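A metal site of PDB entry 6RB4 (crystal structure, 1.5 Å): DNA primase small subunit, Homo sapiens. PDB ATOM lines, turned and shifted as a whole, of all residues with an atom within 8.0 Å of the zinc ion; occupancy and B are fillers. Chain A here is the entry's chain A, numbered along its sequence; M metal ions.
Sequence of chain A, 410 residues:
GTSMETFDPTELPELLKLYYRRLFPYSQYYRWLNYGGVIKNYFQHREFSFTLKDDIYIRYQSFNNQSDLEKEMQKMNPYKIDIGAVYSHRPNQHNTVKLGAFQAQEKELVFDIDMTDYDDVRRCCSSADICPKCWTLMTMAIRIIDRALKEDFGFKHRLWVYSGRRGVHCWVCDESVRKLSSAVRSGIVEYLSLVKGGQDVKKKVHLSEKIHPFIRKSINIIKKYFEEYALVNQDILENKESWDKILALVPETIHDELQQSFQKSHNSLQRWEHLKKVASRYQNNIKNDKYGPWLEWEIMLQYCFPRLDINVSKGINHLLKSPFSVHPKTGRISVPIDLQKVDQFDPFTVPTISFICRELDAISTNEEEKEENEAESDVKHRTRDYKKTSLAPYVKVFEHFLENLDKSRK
Four residues have an atom within 4 Å of the zinc ion: Cys 124, Cys 125, Cys 131 and Cys 134. The nearest printed residue that does not touch the zinc ion is Ile 130 (4.1 Å).
The zinc ion is bound by the side-chain sulfur (SG) of Cys 134 (2.3 Å), the side-chain sulfur (SG) of Cys 124 (2.3 Å), the side-chain sulfur (SG) of Cys 125 (2.3 Å) and the side-chain sulfur (SG) of Cys 131 (2.4 Å).
N of Gly 1 sits close to SG of Cys 125 (3.6 Å). The side-chain sulfur (SG) of Cys 134 lies close to the guanidinium group (NH1) of Arg 122. The side-chain amide nitrogen of Gln 234 lies close to the side-chain sulfur of Cys 124 (3.3 Å). The side-chain sulfur (SG) of Cys 131 lies close to the backbone NH (N) of Lys 133 (3.4 Å).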
ATOM      1  N   GLY A   1     -16.264   9.779 -16.377  1.00  0.00           N
ATOM      2  CA  GLY A   1     -15.607  11.100 -16.198  1.00  0.00           C
ATOM      3  C   GLY A   1     -14.408  11.033 -15.275  1.00  0.00           C
ATOM      4  O   GLY A   1     -13.784   9.988 -15.128  1.00  0.00           O
ATOM      5  N   THR A   2     -14.096  12.159 -14.651  1.00  0.00           N
ATOM      6  CA  THR A   2     -12.936  12.276 -13.773  1.00  0.00           C
ATOM      7  C   THR A   2     -13.288  13.125 -12.571  1.00  0.00           C
ATOM      8  O   THR A   2     -14.142  14.005 -12.654  1.00  0.00           O
ATOM      9  CB  THR A   2     -11.737  12.888 -14.513  1.00  0.00           C
ATOM     10  OG1 THR A   2     -10.625  13.005 -13.615  1.00  0.00           O
ATOM     11  CG2 THR A   2     -12.085  14.277 -15.048  1.00  0.00           C
ATOM     12  N   MET A 115     -22.419  18.793  -8.270  1.00  0.00           N
ATOM     13  CA  MET A 115     -22.822  17.810  -9.283  1.00  0.00           C
ATOM     14  C   MET A 115     -23.397  16.531  -8.676  1.00  0.00           C
ATOM     15  O   MET A 115     -24.238  15.863  -9.326  1.00  0.00           O
ATOM     16  CB  MET A 115     -21.616  17.478 -10.156  1.00  0.00           C
ATOM     17  CG  MET A 115     -22.053  16.706 -11.406  1.00  0.00           C
ATOM     18  SD  MET A 115     -22.898  17.781 -12.587  1.00  0.00           S
ATOM     19  CE  MET A 115     -21.530  18.684 -13.246  1.00  0.00           C
ATOM     20  N   ARG A 122     -27.843  11.551 -14.077  1.00  0.00           N
ATOM     21  CA  ARG A 122     -26.665  11.514 -14.904  1.00  0.00           C
ATOM     22  C   ARG A 122     -26.395  10.085 -15.359  1.00  0.00           C
ATOM     23  O   ARG A 122     -26.388   9.160 -14.546  1.00  0.00           O
ATOM     24  CB  ARG A 122     -25.454  12.049 -14.144  1.00  0.00           C
ATOM     25  CG  ARG A 122     -25.451  13.537 -13.954  1.00  0.00           C
ATOM     26  CD  ARG A 122     -24.063  14.009 -13.553  1.00  0.00           C
ATOM     27  NE  ARG A 122     -23.643  13.449 -12.272  1.00  0.00           N
ATOM     28  CZ  ARG A 122     -22.362  13.323 -11.907  1.00  0.00           C
ATOM     29  NH1 ARG A 122     -21.397  13.724 -12.709  1.00  0.00           N
ATOM     30  NH2 ARG A 122     -22.063  12.822 -10.712  1.00  0.00           N
ATOM     31  N   ARG A 123     -26.201   9.916 -16.656  1.00  0.00           N
ATOM     32  CA  ARG A 123     -25.820   8.612 -17.212  1.00  0.00           C
ATOM     33  C   ARG A 123     -24.346   8.553 -17.596  1.00  0.00           C
ATOM     34  O   ARG A 123     -23.846   7.479 -17.947  1.00  0.00           O
ATOM     35  CB  ARG A 123     -26.685   8.292 -18.439  1.00  0.00           C
ATOM     36  CG  ARG A 123     -28.171   8.198 -18.111  1.00  0.00           C
ATOM     37  CD  ARG A 123     -28.999   7.643 -19.274  1.00  0.00           C
ATOM     38  NE  ARG A 123     -28.659   6.258 -19.592  1.00  0.00           N
ATOM     39  CZ  ARG A 123     -28.190   5.826 -20.764  1.00  0.00           C
ATOM     40  NH1 ARG A 123     -28.020   6.666 -21.787  1.00  0.00           N
ATOM     41  NH2 ARG A 123     -27.915   4.540 -20.927  1.00  0.00           N
ATOM     42  N   CYS A 124     -23.633   9.667 -17.547  1.00  0.00           N
ATOM     43  CA  CYS A 124     -22.297   9.766 -18.066  1.00  0.00           C
ATOM     44  C   CYS A 124     -21.226   9.403 -17.037  1.00  0.00           C
ATOM     45  O   CYS A 124     -20.248   8.716 -17.387  1.00  0.00           O
ATOM     46  CB  CYS A 124     -22.054  11.202 -18.570  1.00  0.00           C
ATOM     47  SG  CYS A 124     -22.553  12.469 -17.330  1.00  0.00           S
ATOM     48  N   CYS A 125     -21.371   9.876 -15.794  1.00  0.00           N
ATOM     49  CA  CYS A 125     -20.318   9.811 -14.800  1.00  0.00           C
ATOM     50  C   CYS A 125     -20.777   9.108 -13.531  1.00  0.00           C
ATOM     51  O   CYS A 125     -21.932   9.226 -13.110  1.00  0.00           O
ATOM     52  CB  CYS A 125     -19.841  11.222 -14.419  1.00  0.00           C
ATOM     53  SG  CYS A 125     -18.995  12.079 -15.657  1.00  0.00           S
ATOM     54  N   SER A 126     -19.820   8.446 -12.882  1.00  0.00           N
ATOM     55  CA  SER A 126     -20.004   8.001 -11.511  1.00  0.00           C
ATOM     56  C   SER A 126     -20.106   9.219 -10.589  1.00  0.00           C
ATOM     57  O   SER A 126     -19.757  10.333 -10.960  1.00  0.00           O
ATOM     58  CB  SER A 126     -18.825   7.111 -11.075  1.00  0.00           C
ATOM     59  OG  SER A 126     -18.656   6.010 -11.969  1.00  0.00           O
ATOM     60  N   ASP A 129     -17.380  11.957 -10.181  1.00  0.00           N
ATOM     61  CA  ASP A 129     -16.745  12.428 -11.406  1.00  0.00           C
ATOM     62  C   ASP A 129     -17.590  13.495 -12.111  1.00  0.00           C
ATOM     63  O   ASP A 129     -18.801  13.616 -11.874  1.00  0.00           O
ATOM     64  CB  ASP A 129     -16.518  11.247 -12.352  1.00  0.00           C
ATOM     65  CG  ASP A 129     -15.584  10.180 -11.764  1.00  0.00           C
ATOM     66  OD1 ASP A 129     -14.750  10.529 -10.928  1.00  0.00           O
ATOM     67  OD2 ASP A 129     -15.698   9.003 -12.173  1.00  0.00           O
ATOM     68  N   ILE A 130     -16.925  14.239 -13.003  1.00  0.00           N
ATOM     69  CA  ILE A 130     -17.607  15.120 -13.936  1.00  0.00           C
ATOM     70  C   ILE A 130     -17.028  14.937 -15.337  1.00  0.00           C
ATOM     71  O   ILE A 130     -15.921  14.387 -15.521  1.00  0.00           O
ATOM     72  CB  ILE A 130     -17.549  16.610 -13.525  1.00  0.00           C
ATOM     73  CG1 ILE A 130     -16.122  17.125 -13.565  1.00  0.00           C
ATOM     74  CG2 ILE A 130     -18.167  16.796 -12.139  1.00  0.00           C
ATOM     75  CD1 ILE A 130     -16.026  18.650 -13.518  1.00  0.00           C
ATOM     76  N   CYS A 131     -17.739  15.465 -16.325  1.00  0.00           N
ATOM     77  CA  CYS A 131     -17.310  15.400 -17.708  1.00  0.00           C
ATOM     78  C   CYS A 131     -17.953  16.541 -18.487  1.00  0.00           C
ATOM     79  O   CYS A 131     -18.803  17.282 -17.946  1.00  0.00           O
ATOM     80  CB  CYS A 131     -17.667  14.044 -18.331  1.00  0.00           C
ATOM     81  SG  CYS A 131     -19.377  13.867 -18.787  1.00  0.00           S
ATOM     82  N   PRO A 132     -17.567  16.748 -19.742  1.00  0.00           N
ATOM     83  CA  PRO A 132     -18.146  17.863 -20.522  1.00  0.00           C
ATOM     84  C   PRO A 132     -19.642  17.731 -20.737  1.00  0.00           C
ATOM     85  O   PRO A 132     -20.307  18.745 -20.974  1.00  0.00           O
ATOM     86  CB  PRO A 132     -17.387  17.795 -21.858  1.00  0.00           C
ATOM     87  CG  PRO A 132     -16.049  17.191 -21.469  1.00  0.00           C
ATOM     88  CD  PRO A 132     -16.410  16.137 -20.458  1.00  0.00           C
ATOM     89  N   LYS A 133     -20.194  16.538 -20.637  1.00  0.00           N
ATOM     90  CA  LYS A 133     -21.631  16.352 -20.753  1.00  0.00           C
ATOM     91  C   LYS A 133     -22.341  16.937 -19.542  1.00  0.00           C
ATOM     92  O   LYS A 133     -23.159  17.866 -19.661  1.00  0.00           O
ATOM     93  CB  LYS A 133     -21.991  14.880 -20.889  1.00  0.00           C
ATOM     94  CG  LYS A 133     -21.491  14.202 -22.127  1.00  0.00           C
ATOM     95  CD  LYS A 133     -22.042  12.783 -22.192  1.00  0.00           C
ATOM     96  CE  LYS A 133     -21.629  12.058 -23.453  1.00  0.00           C
ATOM     97  NZ  LYS A 133     -22.283  10.710 -23.521  1.00  0.00           N
ATOM     98  N   CYS A 134     -22.030  16.428 -18.364  1.00  0.00           N
ATOM     99  CA  CYS A 134     -22.802  16.852 -17.204  1.00  0.00           C
ATOM    100  C   CYS A 134     -22.456  18.261 -16.746  1.00  0.00           C
ATOM    101  O   CYS A 134     -23.224  18.856 -15.964  1.00  0.00           O
ATOM    102  CB  CYS A 134     -22.697  15.879 -16.033  1.00  0.00           C
ATOM    103  SG  CYS A 134     -21.036  15.308 -15.587  1.00  0.00           S
ATOM    104  N   TRP A 135     -21.369  18.866 -17.231  1.00  0.00           N
ATOM    105  CA  TRP A 135     -21.113  20.250 -16.851  1.00  0.00           C
ATOM    106  C   TRP A 135     -22.233  21.174 -17.358  1.00  0.00           C
ATOM    107  O   TRP A 135     -22.488  22.226 -16.762  1.00  0.00           O
ATOM    108  CB  TRP A 135     -19.754  20.748 -17.346  1.00  0.00           C
ATOM    109  CG  TRP A 135     -19.508  22.102 -16.706  1.00  0.00           C
ATOM    110  CD1 TRP A 135     -19.651  23.289 -17.290  1.00  0.00           C
ATOM    111  CD2 TRP A 135     -19.145  22.317 -15.361  1.00  0.00           C
ATOM    112  NE1 TRP A 135     -19.427  24.293 -16.374  1.00  0.00           N
ATOM    113  CE2 TRP A 135     -19.127  23.711 -15.176  1.00  0.00           C
ATOM    114  CE3 TRP A 135     -18.899  21.479 -14.278  1.00  0.00           C
ATOM    115  CZ2 TRP A 135     -18.810  24.313 -13.940  1.00  0.00           C
ATOM    116  CZ3 TRP A 135     -18.584  22.067 -13.048  1.00  0.00           C
ATOM    117  CH2 TRP A 135     -18.563  23.470 -12.894  1.00  0.00           C
ATOM    118  N   THR A 136     -22.949  20.783 -18.419  1.00  0.00           N
ATOM    119  CA  THR A 136     -24.070  21.576 -18.904  1.00  0.00           C
ATOM    120  C   THR A 136     -25.106  21.785 -17.826  1.00  0.00           C
ATOM    121  O   THR A 136     -25.834  22.770 -17.862  1.00  0.00           O
ATOM    122  CB  THR A 136     -24.710  20.900 -20.116  1.00  0.00           C
ATOM    123  OG1 THR A 136     -23.700  20.462 -21.025  1.00  0.00           O
ATOM    124  CG2 THR A 136     -25.633  21.845 -20.838  1.00  0.00           C
ATOM    125  N   LEU A 137     -25.207  20.857 -16.871  1.00  0.00           N
ATOM    126  CA  LEU A 137     -26.130  21.065 -15.755  1.00  0.00           C
ATOM    127  C   LEU A 137     -25.778  22.333 -14.995  1.00  0.00           C
ATOM    128  O   LEU A 137     -26.682  23.080 -14.568  1.00  0.00           O
ATOM    129  CB  LEU A 137     -26.089  19.881 -14.799  1.00  0.00           C
ATOM    130  CG  LEU A 137     -26.688  18.593 -15.358  1.00  0.00           C
ATOM    131  CD1 LEU A 137     -26.370  17.408 -14.459  1.00  0.00           C
ATOM    132  CD2 LEU A 137     -28.226  18.699 -15.532  1.00  0.00           C
ATOM    133  N   TYR A 229     -28.317  18.302 -24.727  1.00  0.00           N
ATOM    134  CA  TYR A 229     -27.876  17.766 -23.448  1.00  0.00           C
ATOM    135  C   TYR A 229     -28.558  16.445 -23.132  1.00  0.00           C
ATOM    136  O   TYR A 229     -27.902  15.447 -22.817  1.00  0.00           O
ATOM    137  CB  TYR A 229     -28.148  18.791 -22.304  1.00  0.00           C
ATOM    138  CG  TYR A 229     -27.961  18.106 -20.971  1.00  0.00           C
ATOM    139  CD1 TYR A 229     -26.665  17.768 -20.537  1.00  0.00           C
ATOM    140  CD2 TYR A 229     -29.016  17.709 -20.198  1.00  0.00           C
ATOM    141  CE1 TYR A 229     -26.472  17.098 -19.357  1.00  0.00           C
ATOM    142  CE2 TYR A 229     -28.850  17.050 -19.007  1.00  0.00           C
ATOM    143  CZ  TYR A 229     -27.536  16.728 -18.591  1.00  0.00           C
ATOM    144  OH  TYR A 229     -27.346  16.038 -17.433  1.00  0.00           O
ATOM    145  N   GLN A 234     -26.819  12.805 -23.038  1.00  0.00           N
ATOM    146  CA  GLN A 234     -27.231  11.855 -22.022  1.00  0.00           C
ATOM    147  C   GLN A 234     -28.028  10.687 -22.589  1.00  0.00           C
ATOM    148  O   GLN A 234     -28.120   9.645 -21.924  1.00  0.00           O
ATOM    149  CB  GLN A 234     -28.079  12.550 -20.947  1.00  0.00           C
ATOM    150  CG  GLN A 234     -27.317  13.572 -20.109  1.00  0.00           C
ATOM    151  CD  GLN A 234     -26.222  12.944 -19.247  1.00  0.00           C
ATOM    152  OE1 GLN A 234     -26.334  11.823 -18.781  1.00  0.00           O
ATOM    153  NE2 GLN A 234     -25.162  13.685 -19.040  1.00  0.00           N
ATOM    154  N   PHE A 348     -12.316  22.064 -16.968  1.00  0.00           N
ATOM    155  CA  PHE A 348     -11.069  21.386 -17.243  1.00  0.00           C
ATOM    156  C   PHE A 348      -9.977  22.316 -17.740  1.00  0.00           C
ATOM    157  O   PHE A 348      -8.806  21.877 -17.820  1.00  0.00           O
ATOM    158  CB  PHE A 348     -11.344  20.236 -18.239  1.00  0.00           C
ATOM    159  CG  PHE A 348     -12.352  19.278 -17.758  1.00  0.00           C
ATOM    160  CD1 PHE A 348     -12.112  18.471 -16.658  1.00  0.00           C
ATOM    161  CD2 PHE A 348     -13.606  19.200 -18.350  1.00  0.00           C
ATOM    162  CE1 PHE A 348     -13.072  17.601 -16.184  1.00  0.00           C
ATOM    163  CE2 PHE A 348     -14.561  18.329 -17.889  1.00  0.00           C
ATOM    164  CZ  PHE A 348     -14.303  17.526 -16.813  1.00  0.00           C
HETATM  165 ZN    ZN M   1     -20.528  13.444 -16.755  1.00  0.00          ZN
